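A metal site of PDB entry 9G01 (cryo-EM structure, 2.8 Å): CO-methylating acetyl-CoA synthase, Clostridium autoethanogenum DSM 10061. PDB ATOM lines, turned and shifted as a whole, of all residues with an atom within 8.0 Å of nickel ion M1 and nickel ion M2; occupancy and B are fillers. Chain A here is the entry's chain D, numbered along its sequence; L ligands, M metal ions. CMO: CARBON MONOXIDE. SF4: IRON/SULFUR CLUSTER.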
ATOM      1  N   ARG A 121     -29.534 -13.401 -15.640  1.00  0.00           N
ATOM      2  CA  ARG A 121     -30.203 -12.406 -16.471  1.00  0.00           C
ATOM      3  C   ARG A 121     -31.277 -11.664 -15.689  1.00  0.00           C
ATOM      4  O   ARG A 121     -31.548 -10.485 -15.979  1.00  0.00           O
ATOM      5  CB  ARG A 121     -30.811 -13.076 -17.694  1.00  0.00           C
ATOM      6  CG  ARG A 121     -29.820 -13.848 -18.545  1.00  0.00           C
ATOM      7  CD  ARG A 121     -30.498 -14.505 -19.731  1.00  0.00           C
ATOM      8  NE  ARG A 121     -29.647 -15.478 -20.400  1.00  0.00           N
ATOM      9  CZ  ARG A 121     -28.852 -15.204 -21.431  1.00  0.00           C
ATOM     10  NH1 ARG A 121     -28.788 -13.992 -21.959  1.00  0.00           N
ATOM     11  NH2 ARG A 121     -28.108 -16.181 -21.939  1.00  0.00           N
ATOM     12  N   GLY A 124     -29.531  -9.050 -13.960  1.00  0.00           N
ATOM     13  CA  GLY A 124     -28.722  -8.216 -14.825  1.00  0.00           C
ATOM     14  C   GLY A 124     -29.168  -6.771 -14.843  1.00  0.00           C
ATOM     15  O   GLY A 124     -28.350  -5.854 -14.813  1.00  0.00           O
ATOM     16  N   VAL A 125     -30.480  -6.532 -14.905  1.00  0.00           N
ATOM     17  CA  VAL A 125     -31.043  -5.174 -14.896  1.00  0.00           C
ATOM     18  C   VAL A 125     -30.698  -4.461 -13.595  1.00  0.00           C
ATOM     19  O   VAL A 125     -30.139  -3.361 -13.619  1.00  0.00           O
ATOM     20  CB  VAL A 125     -32.537  -5.176 -15.184  1.00  0.00           C
ATOM     21  CG1 VAL A 125     -33.144  -3.823 -14.843  1.00  0.00           C
ATOM     22  CG2 VAL A 125     -32.776  -5.496 -16.644  1.00  0.00           C
ATOM     23  N   VAL A 128     -27.369  -3.025 -13.752  1.00  0.00           N
ATOM     24  CA  VAL A 128     -27.181  -1.863 -14.644  1.00  0.00           C
ATOM     25  C   VAL A 128     -27.864  -0.616 -14.097  1.00  0.00           C
ATOM     26  O   VAL A 128     -27.338   0.495 -14.219  1.00  0.00           O
ATOM     27  CB  VAL A 128     -27.605  -2.137 -16.112  1.00  0.00           C
ATOM     28  CG1 VAL A 128     -26.728  -3.208 -16.730  1.00  0.00           C
ATOM     29  CG2 VAL A 128     -29.078  -2.455 -16.283  1.00  0.00           C
ATOM     30  N   ILE A 208     -22.392 -13.170 -21.132  1.00  0.00           N
ATOM     31  CA  ILE A 208     -23.767 -12.831 -21.510  1.00  0.00           C
ATOM     32  C   ILE A 208     -23.876 -11.363 -21.897  1.00  0.00           C
ATOM     33  O   ILE A 208     -24.251 -11.028 -23.025  1.00  0.00           O
ATOM     34  CB  ILE A 208     -24.736 -13.167 -20.357  1.00  0.00           C
ATOM     35  CG1 ILE A 208     -24.812 -14.691 -20.164  1.00  0.00           C
ATOM     36  CG2 ILE A 208     -26.120 -12.596 -20.627  1.00  0.00           C
ATOM     37  CD1 ILE A 208     -25.608 -15.123 -18.951  1.00  0.00           C
ATOM     38  N   PHE A 209     -23.557 -10.467 -20.966  1.00  0.00           N
ATOM     39  CA  PHE A 209     -23.770  -9.043 -21.218  1.00  0.00           C
ATOM     40  C   PHE A 209     -22.624  -8.443 -22.012  1.00  0.00           C
ATOM     41  O   PHE A 209     -22.851  -7.602 -22.886  1.00  0.00           O
ATOM     42  CB  PHE A 209     -23.947  -8.295 -19.899  1.00  0.00           C
ATOM     43  CG  PHE A 209     -25.009  -8.883 -19.025  1.00  0.00           C
ATOM     44  CD1 PHE A 209     -26.337  -8.833 -19.394  1.00  0.00           C
ATOM     45  CD2 PHE A 209     -24.679  -9.467 -17.826  1.00  0.00           C
ATOM     46  CE1 PHE A 209     -27.315  -9.357 -18.584  1.00  0.00           C
ATOM     47  CE2 PHE A 209     -25.649  -9.997 -17.007  1.00  0.00           C
ATOM     48  CZ  PHE A 209     -26.966  -9.948 -17.395  1.00  0.00           C
ATOM     49  N   LEU A 487     -28.902   2.704 -21.096  1.00  0.00           N
ATOM     50  CA  LEU A 487     -28.655   2.363 -19.697  1.00  0.00           C
ATOM     51  C   LEU A 487     -27.878   1.060 -19.589  1.00  0.00           C
ATOM     52  O   LEU A 487     -26.975   0.946 -18.750  1.00  0.00           O
ATOM     53  CB  LEU A 487     -29.989   2.270 -18.944  1.00  0.00           C
ATOM     54  CG  LEU A 487     -29.866   2.026 -17.431  1.00  0.00           C
ATOM     55  CD1 LEU A 487     -29.067   3.132 -16.734  1.00  0.00           C
ATOM     56  CD2 LEU A 487     -31.256   1.904 -16.823  1.00  0.00           C
ATOM     57  N   CYS A 488     -28.203   0.085 -20.419  1.00  0.00           N
ATOM     58  CA  CYS A 488     -27.547  -1.225 -20.365  1.00  0.00           C
ATOM     59  C   CYS A 488     -26.145  -1.219 -20.931  1.00  0.00           C
ATOM     60  O   CYS A 488     -25.545  -2.288 -21.042  1.00  0.00           O
ATOM     61  CB  CYS A 488     -28.384  -2.268 -21.115  1.00  0.00           C
ATOM     62  SG  CYS A 488     -29.804  -2.894 -20.182  1.00  0.00           S
ATOM     63  N   GLN A 489     -25.580  -0.065 -21.288  1.00  0.00           N
ATOM     64  CA  GLN A 489     -24.212   0.001 -21.778  1.00  0.00           C
ATOM     65  C   GLN A 489     -23.179  -0.180 -20.680  1.00  0.00           C
ATOM     66  O   GLN A 489     -21.997  -0.387 -20.991  1.00  0.00           O
ATOM     67  CB  GLN A 489     -23.951   1.316 -22.494  1.00  0.00           C
ATOM     68  CG  GLN A 489     -24.502   1.354 -23.919  1.00  0.00           C
ATOM     69  CD  GLN A 489     -23.948   2.520 -24.733  1.00  0.00           C
ATOM     70  OE1 GLN A 489     -24.236   2.629 -25.919  1.00  0.00           O
ATOM     71  NE2 GLN A 489     -23.152   3.389 -24.095  1.00  0.00           N
ATOM     72  N   SER A 490     -23.588  -0.092 -19.410  1.00  0.00           N
ATOM     73  CA  SER A 490     -22.637  -0.354 -18.333  1.00  0.00           C
ATOM     74  C   SER A 490     -22.143  -1.792 -18.341  1.00  0.00           C
ATOM     75  O   SER A 490     -21.107  -2.082 -17.724  1.00  0.00           O
ATOM     76  CB  SER A 490     -23.296   0.001 -16.983  1.00  0.00           C
ATOM     77  OG  SER A 490     -22.448  -0.332 -15.891  1.00  0.00           O
ATOM     78  N   PHE A 491     -22.885  -2.712 -18.964  1.00  0.00           N
ATOM     79  CA  PHE A 491     -22.469  -4.099 -19.101  1.00  0.00           C
ATOM     80  C   PHE A 491     -22.387  -4.598 -20.535  1.00  0.00           C
ATOM     81  O   PHE A 491     -21.648  -5.545 -20.804  1.00  0.00           O
ATOM     82  CB  PHE A 491     -23.395  -5.044 -18.305  1.00  0.00           C
ATOM     83  CG  PHE A 491     -22.999  -5.212 -16.867  1.00  0.00           C
ATOM     84  CD1 PHE A 491     -22.843  -4.103 -16.035  1.00  0.00           C
ATOM     85  CD2 PHE A 491     -22.788  -6.488 -16.337  1.00  0.00           C
ATOM     86  CE1 PHE A 491     -22.476  -4.253 -14.685  1.00  0.00           C
ATOM     87  CE2 PHE A 491     -22.412  -6.664 -14.990  1.00  0.00           C
ATOM     88  CZ  PHE A 491     -22.261  -5.542 -14.157  1.00  0.00           C
ATOM     89  N   ALA A 492     -23.102  -3.963 -21.475  1.00  0.00           N
ATOM     90  CA  ALA A 492     -23.062  -4.274 -22.893  1.00  0.00           C
ATOM     91  C   ALA A 492     -22.697  -3.010 -23.668  1.00  0.00           C
ATOM     92  O   ALA A 492     -23.584  -2.257 -24.100  1.00  0.00           O
ATOM     93  CB  ALA A 492     -24.407  -4.833 -23.372  1.00  0.00           C
ATOM     94  N   HIS A 495     -24.539  -2.200 -27.109  1.00  0.00           N
ATOM     95  CA  HIS A 495     -25.988  -2.341 -27.181  1.00  0.00           C
ATOM     96  C   HIS A 495     -26.670  -0.999 -26.956  1.00  0.00           C
ATOM     97  O   HIS A 495     -26.405  -0.317 -25.956  1.00  0.00           O
ATOM     98  CB  HIS A 495     -26.479  -3.342 -26.137  1.00  0.00           C
ATOM     99  CG  HIS A 495     -27.962  -3.301 -25.934  1.00  0.00           C
ATOM    100  ND1 HIS A 495     -28.862  -3.589 -26.931  1.00  0.00           N
ATOM    101  CD2 HIS A 495     -28.709  -2.977 -24.847  1.00  0.00           C
ATOM    102  CE1 HIS A 495     -30.093  -3.451 -26.486  1.00  0.00           C
ATOM    103  NE2 HIS A 495     -30.029  -3.086 -25.207  1.00  0.00           N
ATOM    104  N   CYS A 497     -30.747   0.538 -27.227  1.00  0.00           N
ATOM    105  CA  CYS A 497     -32.169   0.310 -27.459  1.00  0.00           C
ATOM    106  C   CYS A 497     -32.795   1.507 -28.152  1.00  0.00           C
ATOM    107  O   CYS A 497     -32.317   2.637 -28.017  1.00  0.00           O
ATOM    108  CB  CYS A 497     -32.910   0.058 -26.142  1.00  0.00           C
ATOM    109  SG  CYS A 497     -32.818  -1.644 -25.564  1.00  0.00           S
ATOM    110  N   LEU A 506     -36.398  -3.974 -24.482  1.00  0.00           N
ATOM    111  CA  LEU A 506     -36.407  -5.430 -24.367  1.00  0.00           C
ATOM    112  C   LEU A 506     -36.386  -5.887 -22.917  1.00  0.00           C
ATOM    113  O   LEU A 506     -36.848  -7.000 -22.623  1.00  0.00           O
ATOM    114  CB  LEU A 506     -35.242  -6.038 -25.156  1.00  0.00           C
ATOM    115  CG  LEU A 506     -33.822  -5.592 -24.800  1.00  0.00           C
ATOM    116  CD1 LEU A 506     -33.102  -6.645 -23.966  1.00  0.00           C
ATOM    117  CD2 LEU A 506     -33.053  -5.314 -26.073  1.00  0.00           C
ATOM    118  N   CYS A 507     -35.898  -5.054 -22.005  1.00  0.00           N
ATOM    119  CA  CYS A 507     -35.981  -5.385 -20.584  1.00  0.00           C
ATOM    120  C   CYS A 507     -37.420  -5.366 -20.073  1.00  0.00           C
ATOM    121  O   CYS A 507     -37.711  -6.004 -19.061  1.00  0.00           O
ATOM    122  CB  CYS A 507     -35.107  -4.439 -19.760  1.00  0.00           C
ATOM    123  SG  CYS A 507     -35.688  -2.735 -19.802  1.00  0.00           S
ATOM    124  N   THR A 572     -29.974  -4.929 -31.543  1.00  0.00           N
ATOM    125  CA  THR A 572     -29.236  -5.802 -30.644  1.00  0.00           C
ATOM    126  C   THR A 572     -29.951  -5.918 -29.298  1.00  0.00           C
ATOM    127  O   THR A 572     -30.752  -5.058 -28.906  1.00  0.00           O
ATOM    128  CB  THR A 572     -27.807  -5.292 -30.432  1.00  0.00           C
ATOM    129  OG1 THR A 572     -27.815  -3.951 -29.934  1.00  0.00           O
ATOM    130  CG2 THR A 572     -27.038  -5.323 -31.730  1.00  0.00           C
ATOM    131  N   SER A 573     -29.647  -7.003 -28.587  1.00  0.00           N
ATOM    132  CA  SER A 573     -30.074  -7.219 -27.221  1.00  0.00           C
ATOM    133  C   SER A 573     -28.844  -7.484 -26.385  1.00  0.00           C
ATOM    134  O   SER A 573     -27.773  -7.791 -26.919  1.00  0.00           O
ATOM    135  CB  SER A 573     -31.042  -8.422 -27.092  1.00  0.00           C
ATOM    136  OG  SER A 573     -32.173  -8.292 -27.952  1.00  0.00           O
ATOM    137  N   CYS A 574     -28.958  -7.355 -25.056  1.00  0.00           N
ATOM    138  CA  CYS A 574     -27.806  -7.493 -24.190  1.00  0.00           C
ATOM    139  C   CYS A 574     -27.940  -8.774 -23.377  1.00  0.00           C
ATOM    140  O   CYS A 574     -27.210  -9.741 -23.640  1.00  0.00           O
ATOM    141  CB  CYS A 574     -27.690  -6.257 -23.287  1.00  0.00           C
ATOM    142  SG  CYS A 574     -29.308  -5.695 -22.723  1.00  0.00           S
ATOM    143  N   GLY A 575     -28.810  -8.820 -22.378  1.00  0.00           N
ATOM    144  CA  GLY A 575     -29.044 -10.076 -21.680  1.00  0.00           C
ATOM    145  C   GLY A 575     -30.363 -10.145 -20.946  1.00  0.00           C
ATOM    146  O   GLY A 575     -30.656 -11.130 -20.268  1.00  0.00           O
ATOM    147  N   CYS A 576     -31.186  -9.107 -21.084  1.00  0.00           N
ATOM    148  CA  CYS A 576     -32.290  -8.846 -20.170  1.00  0.00           C
ATOM    149  C   CYS A 576     -33.664  -9.004 -20.800  1.00  0.00           C
ATOM    150  O   CYS A 576     -34.672  -8.703 -20.160  1.00  0.00           O
ATOM    151  CB  CYS A 576     -32.140  -7.434 -19.590  1.00  0.00           C
ATOM    152  SG  CYS A 576     -31.802  -6.202 -20.876  1.00  0.00           S
ATOM    153  N   PHE A 577     -33.723  -9.495 -22.037  1.00  0.00           N
ATOM    154  CA  PHE A 577     -35.010  -9.635 -22.711  1.00  0.00           C
ATOM    155  C   PHE A 577     -35.903 -10.620 -21.978  1.00  0.00           C
ATOM    156  O   PHE A 577     -35.452 -11.688 -21.560  1.00  0.00           O
ATOM    157  CB  PHE A 577     -34.798 -10.067 -24.166  1.00  0.00           C
ATOM    158  CG  PHE A 577     -33.674 -11.033 -24.356  1.00  0.00           C
ATOM    159  CD1 PHE A 577     -33.869 -12.393 -24.186  1.00  0.00           C
ATOM    160  CD2 PHE A 577     -32.395 -10.569 -24.679  1.00  0.00           C
ATOM    161  CE1 PHE A 577     -32.812 -13.305 -24.348  1.00  0.00           C
ATOM    162  CE2 PHE A 577     -31.334 -11.448 -24.845  1.00  0.00           C
ATOM    163  CZ  PHE A 577     -31.533 -12.823 -24.681  1.00  0.00           C
ATOM    164  N   GLU A 578     -37.165 -10.232 -21.796  1.00  0.00           N
ATOM    165  CA  GLU A 578     -38.128 -11.102 -21.129  1.00  0.00           C
ATOM    166  C   GLU A 578     -38.390 -12.361 -21.941  1.00  0.00           C
ATOM    167  O   GLU A 578     -38.441 -13.465 -21.389  1.00  0.00           O
ATOM    168  CB  GLU A 578     -39.434 -10.341 -20.897  1.00  0.00           C
ATOM    169  CG  GLU A 578     -39.266  -9.104 -20.028  1.00  0.00           C
ATOM    170  CD  GLU A 578     -40.553  -8.314 -19.939  1.00  0.00           C
ATOM    171  OE1 GLU A 578     -41.362  -8.417 -20.878  1.00  0.00           O
ATOM    172  OE2 GLU A 578     -40.778  -7.605 -18.932  1.00  0.00           O
ATOM    173  N   ARG A 595     -38.299 -16.099 -20.129  1.00  0.00           N
ATOM    174  CA  ARG A 595     -37.234 -16.471 -19.206  1.00  0.00           C
ATOM    175  C   ARG A 595     -37.740 -17.450 -18.145  1.00  0.00           C
ATOM    176  O   ARG A 595     -37.010 -18.351 -17.730  1.00  0.00           O
ATOM    177  CB  ARG A 595     -36.628 -15.233 -18.549  1.00  0.00           C
ATOM    178  CG  ARG A 595     -35.546 -15.584 -17.515  1.00  0.00           C
ATOM    179  CD  ARG A 595     -34.442 -14.520 -17.445  1.00  0.00           C
ATOM    180  NE  ARG A 595     -34.919 -13.256 -16.900  1.00  0.00           N
ATOM    181  CZ  ARG A 595     -35.064 -12.131 -17.578  1.00  0.00           C
ATOM    182  NH1 ARG A 595     -34.749 -12.046 -18.857  1.00  0.00           N
ATOM    183  NH2 ARG A 595     -35.507 -11.042 -16.953  1.00  0.00           N
ATOM    184  N   THR A 614     -28.019 -14.464 -28.904  1.00  0.00           N
ATOM    185  CA  THR A 614     -28.383 -13.155 -29.426  1.00  0.00           C
ATOM    186  C   THR A 614     -28.072 -12.007 -28.467  1.00  0.00           C
ATOM    187  O   THR A 614     -28.671 -10.938 -28.604  1.00  0.00           O
ATOM    188  CB  THR A 614     -29.873 -13.122 -29.789  1.00  0.00           C
ATOM    189  OG1 THR A 614     -30.220 -11.848 -30.346  1.00  0.00           O
ATOM    190  CG2 THR A 614     -30.733 -13.375 -28.556  1.00  0.00           C
ATOM    191  N   GLY A 615     -27.144 -12.179 -27.532  1.00  0.00           N
ATOM    192  CA  GLY A 615     -26.854 -11.174 -26.539  1.00  0.00           C
ATOM    193  C   GLY A 615     -25.475 -10.535 -26.708  1.00  0.00           C
ATOM    194  O   GLY A 615     -24.703 -10.864 -27.594  1.00  0.00           O
ATOM    195  N   GLY A 616     -25.199  -9.597 -25.807  1.00  0.00           N
ATOM    196  CA  GLY A 616     -23.918  -8.937 -25.756  1.00  0.00           C
ATOM    197  C   GLY A 616     -23.744  -7.758 -26.697  1.00  0.00           C
ATOM    198  O   GLY A 616     -22.638  -7.221 -26.775  1.00  0.00           O
ATOM    199  N   GLY A 617     -24.791  -7.339 -27.390  1.00  0.00           N
ATOM    200  CA  GLY A 617     -24.670  -6.236 -28.321  1.00  0.00           C
ATOM    201  C   GLY A 617     -24.210  -6.607 -29.705  1.00  0.00           C
ATOM    202  O   GLY A 617     -23.718  -5.738 -30.430  1.00  0.00           O
HETATM  203  C   CMO L   1     -28.616  -5.554 -19.212  1.00  0.00           C
HETATM  204  O   CMO L   1     -27.853  -5.886 -18.293  1.00  0.00           O
HETATM  205 FE1  SF4 L   2     -32.672   0.546 -21.267  1.00  0.00          FE
HETATM  206 FE2  SF4 L   2     -32.631  -1.222 -23.350  1.00  0.00          FE
HETATM  207 FE3  SF4 L   2     -34.181  -1.729 -21.163  1.00  0.00          FE
HETATM  208 FE4  SF4 L   2     -31.455  -1.886 -20.974  1.00  0.00          FE
HETATM  209  S1  SF4 L   2     -32.815  -3.202 -22.241  1.00  0.00           S
HETATM  210  S2  SF4 L   2     -32.876  -0.884 -19.498  1.00  0.00           S
HETATM  211  S3  SF4 L   2     -30.828  -0.206 -22.379  1.00  0.00           S
HETATM  212  S4  SF4 L   2     -34.417  -0.001 -22.619  1.00  0.00           S
HETATM  213 NI    NI M   1     -30.228  -7.538 -21.783  1.00  0.00          NI
HETATM  214 NI    NI M   2     -29.615  -5.129 -20.427  1.00  0.00          NI
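Residues that only touch nickel ion M1: Leu 506 (3.7 Å). The nearest printed residue that does not touch nickel ion M1 is Phe 577 (4.01 Å).
Three residues have an atom within 4 Å of nickel ion M2: Cys 488, Cys 574 and Cys 576.
A sulfur (S3) of SF4 L2 sits close to the backbone NH (N) of Cys 488, at 3.3 Å. SG of Cys 488 binds FE4 of SF4 L2 (2.1 Å). A sulfur (S1) of SF4 L2 lies close to the backbone NH (N) of Cys 507. The side-chain sulfur of Cys 507 is bound to an iron atom (FE3) of SF4 L2, 2.3 Å away. The backbone NH (N) of Leu 487 lies close to a sulfur (S3) of SF4 L2 (3.7 Å). The side-chain sulfur of Cys 497 is bound to an iron atom (FE2) of SF4 L2 (2.3 Å).
Nickel ion M2 is bound by SG of Cys 488 (2.3 Å), SG of Cys 574 (2.4 Å) and SG of Cys 576 (2.5 Å). Nickel ion M2 has three donor atoms within binding distance.
NE2 of His 495 lies close to SG of Cys 574 (3.7 Å). N of Gly 616 is in hydrogen-bond range of O of Cys 574 (3.0 Å). The backbone carbonyl oxygen (O) of Leu 506 lies within hydrogen-bond range of the backbone NH (N) of Glu 578.
Nickel ion M1 is bound by the backbone nitrogen (N) of Cys 576 (2.0 Å). Nickel ion M1 is bound by the backbone nitrogen (N) of Gly 575 (2.0 Å). The side-chain sulfur (SG) of Cys 576 is bound to nickel ion M1. SG of Cys 574 is bound to nickel ion M1 (2.3 Å).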
